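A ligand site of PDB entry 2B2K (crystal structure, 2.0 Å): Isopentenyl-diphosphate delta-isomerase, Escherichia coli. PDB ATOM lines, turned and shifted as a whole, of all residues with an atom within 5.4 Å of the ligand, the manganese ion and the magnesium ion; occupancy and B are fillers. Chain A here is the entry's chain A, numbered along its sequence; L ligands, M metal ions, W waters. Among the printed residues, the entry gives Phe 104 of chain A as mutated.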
ATOM      1  N   GLU A   4      -8.632  -9.497 -17.624  1.00  0.00           N
ATOM      2  CA  GLU A   4      -7.562  -8.755 -18.288  1.00  0.00           C
ATOM      3  C   GLU A   4      -6.275  -9.576 -18.306  1.00  0.00           C
ATOM      4  O   GLU A   4      -5.997 -10.333 -17.369  1.00  0.00           O
ATOM      5  CB  GLU A   4      -7.326  -7.400 -17.618  1.00  0.00           C
ATOM      6  CG  GLU A   4      -6.318  -6.540 -18.359  1.00  0.00           C
ATOM      7  CD  GLU A   4      -6.180  -5.161 -17.738  1.00  0.00           C
ATOM      8  OE1 GLU A   4      -5.543  -4.282 -18.374  1.00  0.00           O
ATOM      9  OE2 GLU A   4      -6.702  -4.973 -16.622  1.00  0.00           O
ATOM     10  N   VAL A   6      -1.985 -10.066 -20.204  1.00  0.00           N
ATOM     11  CA  VAL A   6      -0.883  -9.623 -21.056  1.00  0.00           C
ATOM     12  C   VAL A   6      -0.594 -10.701 -22.110  1.00  0.00           C
ATOM     13  O   VAL A   6      -0.930 -11.868 -21.930  1.00  0.00           O
ATOM     14  CB  VAL A   6       0.401  -9.324 -20.272  1.00  0.00           C
ATOM     15  CG1 VAL A   6       0.041  -8.520 -19.026  1.00  0.00           C
ATOM     16  CG2 VAL A   6       1.158 -10.579 -19.882  1.00  0.00           C
ATOM     17  N   LYS A  21      -3.191 -10.646 -15.899  1.00  0.00           N
ATOM     18  CA  LYS A  21      -2.279  -9.516 -15.765  1.00  0.00           C
ATOM     19  C   LYS A  21      -1.579  -9.500 -14.408  1.00  0.00           C
ATOM     20  O   LYS A  21      -0.368  -9.283 -14.320  1.00  0.00           O
ATOM     21  CB  LYS A  21      -3.002  -8.182 -15.997  1.00  0.00           C
ATOM     22  CG  LYS A  21      -2.044  -6.996 -16.088  1.00  0.00           C
ATOM     23  CD  LYS A  21      -2.743  -5.695 -16.440  1.00  0.00           C
ATOM     24  CE  LYS A  21      -3.349  -5.033 -15.210  1.00  0.00           C
ATOM     25  NZ  LYS A  21      -3.999  -3.740 -15.563  1.00  0.00           N
ATOM     26  N   HIS A  25       3.216 -10.435 -13.588  1.00  0.00           N
ATOM     27  CA  HIS A  25       4.362  -9.640 -13.114  1.00  0.00           C
ATOM     28  C   HIS A  25       4.887 -10.212 -11.799  1.00  0.00           C
ATOM     29  O   HIS A  25       4.247 -10.128 -10.743  1.00  0.00           O
ATOM     30  CB  HIS A  25       3.917  -8.190 -12.980  1.00  0.00           C
ATOM     31  CG  HIS A  25       3.519  -7.579 -14.293  1.00  0.00           C
ATOM     32  ND1 HIS A  25       2.215  -7.528 -14.724  1.00  0.00           N
ATOM     33  CD2 HIS A  25       4.256  -6.997 -15.272  1.00  0.00           C
ATOM     34  CE1 HIS A  25       2.170  -6.939 -15.913  1.00  0.00           C
ATOM     35  NE2 HIS A  25       3.393  -6.606 -16.269  1.00  0.00           N
ATOM     36  N   HIS A  32       6.516  -9.764 -22.631  1.00  0.00           N
ATOM     37  CA  HIS A  32       5.183  -9.561 -23.193  1.00  0.00           C
ATOM     38  C   HIS A  32       5.008  -8.186 -23.837  1.00  0.00           C
ATOM     39  O   HIS A  32       5.894  -7.327 -23.856  1.00  0.00           O
ATOM     40  CB  HIS A  32       4.117  -9.799 -22.112  1.00  0.00           C
ATOM     41  CG  HIS A  32       4.274  -8.924 -20.906  1.00  0.00           C
ATOM     42  ND1 HIS A  32       5.173  -9.154 -19.894  1.00  0.00           N
ATOM     43  CD2 HIS A  32       3.630  -7.783 -20.573  1.00  0.00           C
ATOM     44  CE1 HIS A  32       5.073  -8.211 -18.980  1.00  0.00           C
ATOM     45  NE2 HIS A  32       4.140  -7.363 -19.371  1.00  0.00           N
ATOM     46  N   ALA A  34       3.341  -4.421 -24.447  1.00  0.00           N
ATOM     47  CA  ALA A  34       2.942  -3.248 -23.679  1.00  0.00           C
ATOM     48  C   ALA A  34       2.963  -1.966 -24.486  1.00  0.00           C
ATOM     49  O   ALA A  34       3.301  -1.959 -25.672  1.00  0.00           O
ATOM     50  CB  ALA A  34       3.873  -3.108 -22.476  1.00  0.00           C
ATOM     51  N   PHE A  35       2.625  -0.836 -23.848  1.00  0.00           N
ATOM     52  CA  PHE A  35       2.792   0.457 -24.483  1.00  0.00           C
ATOM     53  C   PHE A  35       3.184   1.483 -23.422  1.00  0.00           C
ATOM     54  O   PHE A  35       2.879   1.243 -22.255  1.00  0.00           O
ATOM     55  CB  PHE A  35       1.559   0.985 -25.222  1.00  0.00           C
ATOM     56  CG  PHE A  35       0.372   1.334 -24.362  1.00  0.00           C
ATOM     57  CD1 PHE A  35       0.137   2.612 -23.867  1.00  0.00           C
ATOM     58  CD2 PHE A  35      -0.533   0.333 -24.032  1.00  0.00           C
ATOM     59  CE1 PHE A  35      -0.941   2.893 -23.061  1.00  0.00           C
ATOM     60  CE2 PHE A  35      -1.630   0.622 -23.240  1.00  0.00           C
ATOM     61  CZ  PHE A  35      -1.847   1.887 -22.763  1.00  0.00           C
ATOM     62  N   SER A  36       3.775   2.562 -23.886  1.00  0.00           N
ATOM     63  CA  SER A  36       4.054   3.737 -23.072  1.00  0.00           C
ATOM     64  C   SER A  36       3.553   4.973 -23.793  1.00  0.00           C
ATOM     65  O   SER A  36       3.712   5.066 -25.018  1.00  0.00           O
ATOM     66  CB  SER A  36       5.547   3.799 -22.762  1.00  0.00           C
ATOM     67  OG  SER A  36       5.919   5.067 -22.242  1.00  0.00           O
ATOM     68  N   ARG A  51       2.540   6.579  -9.777  1.00  0.00           N
ATOM     69  CA  ARG A  51       1.765   5.335  -9.763  1.00  0.00           C
ATOM     70  C   ARG A  51       1.191   5.043  -8.385  1.00  0.00           C
ATOM     71  O   ARG A  51       1.879   5.263  -7.380  1.00  0.00           O
ATOM     72  CB  ARG A  51       2.647   4.180 -10.248  1.00  0.00           C
ATOM     73  CG  ARG A  51       3.039   4.165 -11.722  1.00  0.00           C
ATOM     74  CD  ARG A  51       4.228   3.256 -11.956  1.00  0.00           C
ATOM     75  NE  ARG A  51       3.890   1.834 -11.894  1.00  0.00           N
ATOM     76  CZ  ARG A  51       3.231   1.216 -12.867  1.00  0.00           C
ATOM     77  NH1 ARG A  51       2.855   1.877 -13.948  1.00  0.00           N
ATOM     78  NH2 ARG A  51       2.934  -0.081 -12.771  1.00  0.00           N
ATOM     79  N   LYS A  55      -0.058  -0.425  -7.151  1.00  0.00           N
ATOM     80  CA  LYS A  55       0.378  -1.069  -8.397  1.00  0.00           C
ATOM     81  C   LYS A  55       1.358  -2.189  -8.097  1.00  0.00           C
ATOM     82  O   LYS A  55       2.174  -2.113  -7.177  1.00  0.00           O
ATOM     83  CB  LYS A  55       1.019  -0.074  -9.353  1.00  0.00           C
ATOM     84  CG  LYS A  55       0.064   1.026  -9.814  1.00  0.00           C
ATOM     85  CD  LYS A  55      -1.159   0.466 -10.515  1.00  0.00           C
ATOM     86  CE  LYS A  55      -0.799  -0.410 -11.702  1.00  0.00           C
ATOM     87  NZ  LYS A  55      -2.025  -0.789 -12.472  1.00  0.00           N
ATOM     88  N   ALA A  57       3.915  -3.394  -9.947  1.00  0.00           N
ATOM     89  CA  ALA A  57       5.253  -3.031 -10.386  1.00  0.00           C
ATOM     90  C   ALA A  57       5.474  -1.532 -10.229  1.00  0.00           C
ATOM     91  O   ALA A  57       4.577  -0.771 -10.601  1.00  0.00           O
ATOM     92  CB  ALA A  57       5.490  -3.443 -11.833  1.00  0.00           C
ATOM     93  N   TRP A  58       6.619  -1.130  -9.699  1.00  0.00           N
ATOM     94  CA  TRP A  58       6.975   0.254  -9.417  1.00  0.00           C
ATOM     95  C   TRP A  58       5.865   1.044  -8.757  1.00  0.00           C
ATOM     96  O   TRP A  58       5.472   2.113  -9.222  1.00  0.00           O
ATOM     97  CB  TRP A  58       7.424   0.961 -10.714  1.00  0.00           C
ATOM     98  CG  TRP A  58       8.807   0.526 -11.097  1.00  0.00           C
ATOM     99  CD1 TRP A  58       9.966   1.158 -10.755  1.00  0.00           C
ATOM    100  CD2 TRP A  58       9.191  -0.618 -11.879  1.00  0.00           C
ATOM    101  NE1 TRP A  58      11.046   0.479 -11.277  1.00  0.00           N
ATOM    102  CE2 TRP A  58      10.588  -0.615 -11.969  1.00  0.00           C
ATOM    103  CE3 TRP A  58       8.482  -1.644 -12.514  1.00  0.00           C
ATOM    104  CZ2 TRP A  58      11.314  -1.586 -12.669  1.00  0.00           C
ATOM    105  CZ3 TRP A  58       9.189  -2.606 -13.204  1.00  0.00           C
ATOM    106  CH2 TRP A  58      10.580  -2.580 -13.273  1.00  0.00           C
ATOM    107  N   VAL A  66       0.955   7.641 -19.182  1.00  0.00           N
ATOM    108  CA  VAL A  66       0.090   6.466 -19.106  1.00  0.00           C
ATOM    109  C   VAL A  66       0.775   5.295 -19.789  1.00  0.00           C
ATOM    110  O   VAL A  66       1.302   5.463 -20.896  1.00  0.00           O
ATOM    111  CB  VAL A  66      -1.269   6.766 -19.772  1.00  0.00           C
ATOM    112  CG1 VAL A  66      -1.053   7.232 -21.205  1.00  0.00           C
ATOM    113  CG2 VAL A  66      -2.190   5.559 -19.752  1.00  0.00           C
ATOM    114  N   CYS A  67       0.793   4.144 -19.132  1.00  0.00           N
ATOM    115  CA  CYS A  67       1.368   2.902 -19.633  1.00  0.00           C
ATOM    116  C   CYS A  67       0.378   1.759 -19.448  1.00  0.00           C
ATOM    117  O   CYS A  67      -0.464   1.800 -18.553  1.00  0.00           O
ATOM    118  CB  CYS A  67       2.692   2.572 -18.948  1.00  0.00           C
ATOM    119  SG  CYS A  67       3.909   3.918 -18.943  1.00  0.00           S
ATOM    120  N   GLY A  68       0.467   0.747 -20.302  1.00  0.00           N
ATOM    121  CA  GLY A  68      -0.485  -0.338 -20.275  1.00  0.00           C
ATOM    122  C   GLY A  68      -0.079  -1.527 -21.136  1.00  0.00           C
ATOM    123  O   GLY A  68       1.020  -1.571 -21.681  1.00  0.00           O
ATOM    124  N   HIS A  69      -1.010  -2.467 -21.218  1.00  0.00           N
ATOM    125  CA  HIS A  69      -0.861  -3.765 -21.841  1.00  0.00           C
ATOM    126  C   HIS A  69      -1.969  -4.015 -22.870  1.00  0.00           C
ATOM    127  O   HIS A  69      -3.121  -4.287 -22.507  1.00  0.00           O
ATOM    128  CB  HIS A  69      -0.902  -4.817 -20.734  1.00  0.00           C
ATOM    129  CG  HIS A  69       0.253  -4.835 -19.786  1.00  0.00           C
ATOM    130  ND1 HIS A  69       0.187  -4.282 -18.518  1.00  0.00           N
ATOM    131  CD2 HIS A  69       1.505  -5.358 -19.898  1.00  0.00           C
ATOM    132  CE1 HIS A  69       1.353  -4.453 -17.923  1.00  0.00           C
ATOM    133  NE2 HIS A  69       2.180  -5.106 -18.727  1.00  0.00           N
ATOM    134  N   ARG A  83      -6.513   2.964 -21.829  1.00  0.00           N
ATOM    135  CA  ARG A  83      -5.929   3.202 -20.496  1.00  0.00           C
ATOM    136  C   ARG A  83      -6.002   4.683 -20.132  1.00  0.00           C
ATOM    137  O   ARG A  83      -6.007   5.053 -18.956  1.00  0.00           O
ATOM    138  CB  ARG A  83      -4.506   2.659 -20.444  1.00  0.00           C
ATOM    139  CG  ARG A  83      -4.425   1.142 -20.508  1.00  0.00           C
ATOM    140  CD  ARG A  83      -5.332   0.503 -19.473  1.00  0.00           C
ATOM    141  NE  ARG A  83      -4.761   0.535 -18.123  1.00  0.00           N
ATOM    142  CZ  ARG A  83      -5.335  -0.048 -17.080  1.00  0.00           C
ATOM    143  NH1 ARG A  83      -6.485  -0.701 -17.221  1.00  0.00           N
ATOM    144  NH2 ARG A  83      -4.796  -0.013 -15.864  1.00  0.00           N
ATOM    145  N   GLU A  87      -7.398   5.131 -16.550  1.00  0.00           N
ATOM    146  CA  GLU A  87      -6.503   5.569 -15.485  1.00  0.00           C
ATOM    147  C   GLU A  87      -6.739   7.047 -15.172  1.00  0.00           C
ATOM    148  O   GLU A  87      -6.625   7.462 -14.008  1.00  0.00           O
ATOM    149  CB  GLU A  87      -5.047   5.335 -15.854  1.00  0.00           C
ATOM    150  CG  GLU A  87      -4.680   3.924 -16.282  1.00  0.00           C
ATOM    151  CD  GLU A  87      -3.187   3.707 -16.393  1.00  0.00           C
ATOM    152  OE1 GLU A  87      -2.457   4.716 -16.237  1.00  0.00           O
ATOM    153  OE2 GLU A  87      -2.704   2.566 -16.622  1.00  0.00           O
ATOM    154  N   PHE A 104      12.334  -3.200 -23.219  1.00  0.00           N
ATOM    155  CA  PHE A 104      13.193  -3.190 -22.043  1.00  0.00           C
ATOM    156  C   PHE A 104      12.791  -4.277 -21.041  1.00  0.00           C
ATOM    157  O   PHE A 104      11.708  -4.847 -21.028  1.00  0.00           O
ATOM    158  CB  PHE A 104      13.156  -1.839 -21.311  1.00  0.00           C
ATOM    159  CG  PHE A 104      11.891  -1.719 -20.473  1.00  0.00           C
ATOM    160  CD1 PHE A 104      11.923  -1.763 -19.100  1.00  0.00           C
ATOM    161  CD2 PHE A 104      10.671  -1.558 -21.126  1.00  0.00           C
ATOM    162  CE1 PHE A 104      10.746  -1.653 -18.366  1.00  0.00           C
ATOM    163  CE2 PHE A 104       9.504  -1.451 -20.415  1.00  0.00           C
ATOM    164  CZ  PHE A 104       9.546  -1.501 -19.029  1.00  0.00           C
ATOM    165  N   GLU A 114       9.578  -5.918 -14.915  1.00  0.00           N
ATOM    166  CA  GLU A 114       8.822  -5.724 -16.149  1.00  0.00           C
ATOM    167  C   GLU A 114       9.752  -6.142 -17.299  1.00  0.00           C
ATOM    168  O   GLU A 114      10.959  -5.876 -17.269  1.00  0.00           O
ATOM    169  CB  GLU A 114       8.314  -4.316 -16.394  1.00  0.00           C
ATOM    170  CG  GLU A 114       6.885  -4.044 -15.945  1.00  0.00           C
ATOM    171  CD  GLU A 114       5.813  -4.659 -16.813  1.00  0.00           C
ATOM    172  OE1 GLU A 114       4.623  -4.258 -16.633  1.00  0.00           O
ATOM    173  OE2 GLU A 114       6.043  -5.699 -17.463  1.00  0.00           O
ATOM    174  N   GLU A 116       9.329  -6.137 -21.434  1.00  0.00           N
ATOM    175  CA  GLU A 116       8.317  -5.730 -22.381  1.00  0.00           C
ATOM    176  C   GLU A 116       8.915  -5.291 -23.712  1.00  0.00           C
ATOM    177  O   GLU A 116       9.967  -4.659 -23.789  1.00  0.00           O
ATOM    178  CB  GLU A 116       7.421  -4.600 -21.859  1.00  0.00           C
ATOM    179  CG  GLU A 116       6.888  -4.636 -20.459  1.00  0.00           C
ATOM    180  CD  GLU A 116       5.922  -3.634 -19.898  1.00  0.00           C
ATOM    181  OE1 GLU A 116       6.041  -2.388 -19.794  1.00  0.00           O
ATOM    182  OE2 GLU A 116       4.845  -4.143 -19.443  1.00  0.00           O
ATOM    183  N   CYS A 118       7.730  -2.548 -26.010  1.00  0.00           N
ATOM    184  CA  CYS A 118       6.842  -1.487 -25.510  1.00  0.00           C
ATOM    185  C   CYS A 118       6.854  -0.259 -26.401  1.00  0.00           C
ATOM    186  O   CYS A 118       7.476   0.753 -26.033  1.00  0.00           O
ATOM    187  CB  CYS A 118       7.259  -1.166 -24.068  1.00  0.00           C
ATOM    188  SG  CYS A 118       6.459   0.222 -23.225  1.00  0.00           S
ATOM    189  N   GLU A 135      -5.078   3.695  -9.674  1.00  0.00           N
ATOM    190  CA  GLU A 135      -3.970   3.679 -10.618  1.00  0.00           C
ATOM    191  C   GLU A 135      -2.974   4.828 -10.424  1.00  0.00           C
ATOM    192  O   GLU A 135      -1.761   4.629 -10.495  1.00  0.00           O
ATOM    193  CB  GLU A 135      -4.522   3.710 -12.059  1.00  0.00           C
ATOM    194  CG  GLU A 135      -5.487   2.576 -12.366  1.00  0.00           C
ATOM    195  CD  GLU A 135      -4.802   1.241 -12.581  1.00  0.00           C
ATOM    196  OE1 GLU A 135      -3.598   1.202 -12.914  1.00  0.00           O
ATOM    197  OE2 GLU A 135      -5.455   0.183 -12.416  1.00  0.00           O
ATOM    198  N   TRP A 161      11.996   3.043 -17.365  1.00  0.00           N
ATOM    199  CA  TRP A 161      11.632   3.112 -18.787  1.00  0.00           C
ATOM    200  C   TRP A 161      11.325   4.530 -19.215  1.00  0.00           C
ATOM    201  O   TRP A 161      11.473   4.926 -20.368  1.00  0.00           O
ATOM    202  CB  TRP A 161      10.430   2.207 -19.098  1.00  0.00           C
ATOM    203  CG  TRP A 161       9.212   2.568 -18.309  1.00  0.00           C
ATOM    204  CD1 TRP A 161       8.261   3.489 -18.611  1.00  0.00           C
ATOM    205  CD2 TRP A 161       8.824   1.986 -17.060  1.00  0.00           C
ATOM    206  NE1 TRP A 161       7.299   3.528 -17.625  1.00  0.00           N
ATOM    207  CE2 TRP A 161       7.631   2.604 -16.664  1.00  0.00           C
ATOM    208  CE3 TRP A 161       9.395   0.990 -16.254  1.00  0.00           C
ATOM    209  CZ2 TRP A 161       6.975   2.258 -15.476  1.00  0.00           C
ATOM    210  CZ3 TRP A 161       8.742   0.662 -15.075  1.00  0.00           C
ATOM    211  CH2 TRP A 161       7.552   1.293 -14.698  1.00  0.00           C
HETATM  212  O1  LIG L   1      -1.844  -0.201 -16.300  1.00  0.00           O
HETATM  213  O2  LIG L   1      -1.311  -2.048 -15.020  1.00  0.00           O
HETATM  214  O3  LIG L   1      -2.097  -2.401 -17.211  1.00  0.00           O
HETATM  215  P1  LIG L   1      -1.233  -1.576 -16.285  1.00  0.00           P
HETATM  216  O4  LIG L   1       0.176  -1.515 -16.846  1.00  0.00           O
HETATM  217  O5  LIG L   1       2.144  -1.112 -15.494  1.00  0.00           O
HETATM  218  O6  LIG L   1       0.723   0.699 -16.060  1.00  0.00           O
HETATM  219  P2  LIG L   1       1.349  -0.613 -16.463  1.00  0.00           P
HETATM  220  O7  LIG L   1       2.086  -0.318 -17.768  1.00  0.00           O
HETATM  221  C1  LIG L   1       2.876  -1.417 -18.261  1.00  0.00           C
HETATM  222  C2  LIG L   1       3.796  -1.132 -19.444  1.00  0.00           C
HETATM  223  C3  LIG L   1       5.316  -1.159 -19.057  1.00  0.00           C
HETATM  224  C4  LIG L   1       5.352  -0.753 -17.543  1.00  0.00           C
HETATM  225  C5  LIG L   1       5.928   0.136 -19.713  1.00  0.00           C
HETATM  226  O8  LIG L   1       5.260  -1.911 -16.737  1.00  0.00           O
HETATM  227 MN    MN M   1       3.881  -5.672 -18.036  1.00  0.00          MN
HETATM  228 MG    MG M   2      -0.959   1.684 -16.472  1.00  0.00          MG
HETATM  229  O   HOH W   1      -0.138  -4.575 -14.648  1.00  0.00           O
HETATM  230  O   HOH W   2      -1.259   2.117 -14.657  1.00  0.00           O
HETATM  231  O   HOH W   3      -0.255   3.294 -16.396  1.00  0.00           O
HETATM  232  O   HOH W   4       2.707  -3.762 -14.538  1.00  0.00           O
HETATM  233  O   HOH W   5      -3.139  -1.935 -19.527  1.00  0.00           O
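The side-chain carboxylate (OE1) of Glu 135 is in salt-bridge range of the side-chain amino group (NZ) of Lys 55 (2.6 Å).
NH2 of Arg 51 lies within hydrogen-bond range of O of Ala 57 (2.8 Å).
The guanidinium group (NE) of Arg 51 is in hydrogen-bond range of the backbone carbonyl oxygen (O) of Trp 58, 3.1 Å away.
NE1 of Trp 161 sits at hydrogen-bond distance from SG of Cys 67, at 3.7 Å.
The backbone carbonyl oxygen (O) of Gly 68 lies within hydrogen-bond range of the backbone NH (N) of Phe 35.
The backbone NH (N) of Glu 116 sits at hydrogen-bond distance from the backbone carbonyl oxygen (O) of Phe 104, at 2.7 Å.
The side-chain carboxylate of Glu 87 lies close to the guanidinium group of Arg 83 (3.3 Å).
N of Ser 36 is in hydrogen-bond range of SG of Cys 118 (3.6 Å).
Merely in contact with the ligand: Cys 118 (3.6 Å), Ala 34 (3.6 Å), Phe 35 (3.8 Å), Phe 104 (3.97 Å) and Trp 161 (3.997 Å).
Hydrophobic or aromatic side chains within 4 Å of the ligand: Ala 34, His 69, Phe 104 and Trp 161.
Within 4 Å of the ligand: Lys 21, Ala 34, Phe 35, Arg 51, Lys 55, Cys 67, Gly 68, His 69, Arg 83, Glu 87, Phe 104, Glu 114, Glu 116, Cys 118 and Trp 161.
The manganese ion is bound by NE2 of His 69 (1.9 Å), NE2 of His 25 (2.1 Å), OE1 of Glu 114 (2.1 Å), NE2 of His 32 (2.2 Å), OE2 of Glu 114 (2.2 Å) and OE2 of Glu 116 (2.3 Å).
Water W3 lies within hydrogen-bond range of the side-chain carboxylate of Glu 87 and the backbone NH of Cys 67.
Water W2 lies within hydrogen-bond range of the side-chain carboxylate of Glu 135 (3.1 Å) and the side-chain carboxylate of Glu 87 (3.3 Å).
Water W5 lies within hydrogen-bond range of an oxygen (O3) of the ligand (2.6 Å), the backbone NH of His 69 (2.8 Å) and the guanidinium group of Arg 83 (3.3 Å).
Within 4 Å of the magnesium ion: Cys 67 and Glu 87.
Along chain A the residues within 4 Å of the magnesium ion span positions 67 to 87.
The magnesium ion is bound by water W3 (1.8 Å), water W2 (1.9 Å), the side-chain carboxylate (OE2) of Glu 87 (2.0 Å), an oxygen (O6) of the ligand (2.0 Å), an oxygen (O1) of the ligand (2.1 Å) and the backbone carbonyl oxygen (O) of Cys 67 (2.1 Å).
An oxygen (O5) of the ligand lies within salt-bridge range of the guanidinium group of Arg 51 (3.0 Å).
NZ of Lys 21 lies within salt-bridge range of O3 of the ligand (2.9 Å).
The side-chain carboxylate of Glu 116 is covalently linked to a carbon (C3) of the ligand (1.6 Å).
An oxygen (O7) of the ligand lies within hydrogen-bond range of the backbone NH (N) of Gly 68 (3.2 Å).
The side-chain carboxylate (OE1) of Glu 114 sits close to an oxygen (O8) of the ligand (2.4 Å).
The side-chain amino group (NZ) of Lys 55 lies within salt-bridge range of an oxygen (O2) of the ligand (2.9 Å).
ND1 of His 69 sits at hydrogen-bond distance from O4 of the ligand (3.2 Å).
The guanidinium group (NH2) of Arg 83 lies within salt-bridge range of an oxygen (O3) of the ligand, at 3.8 Å.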
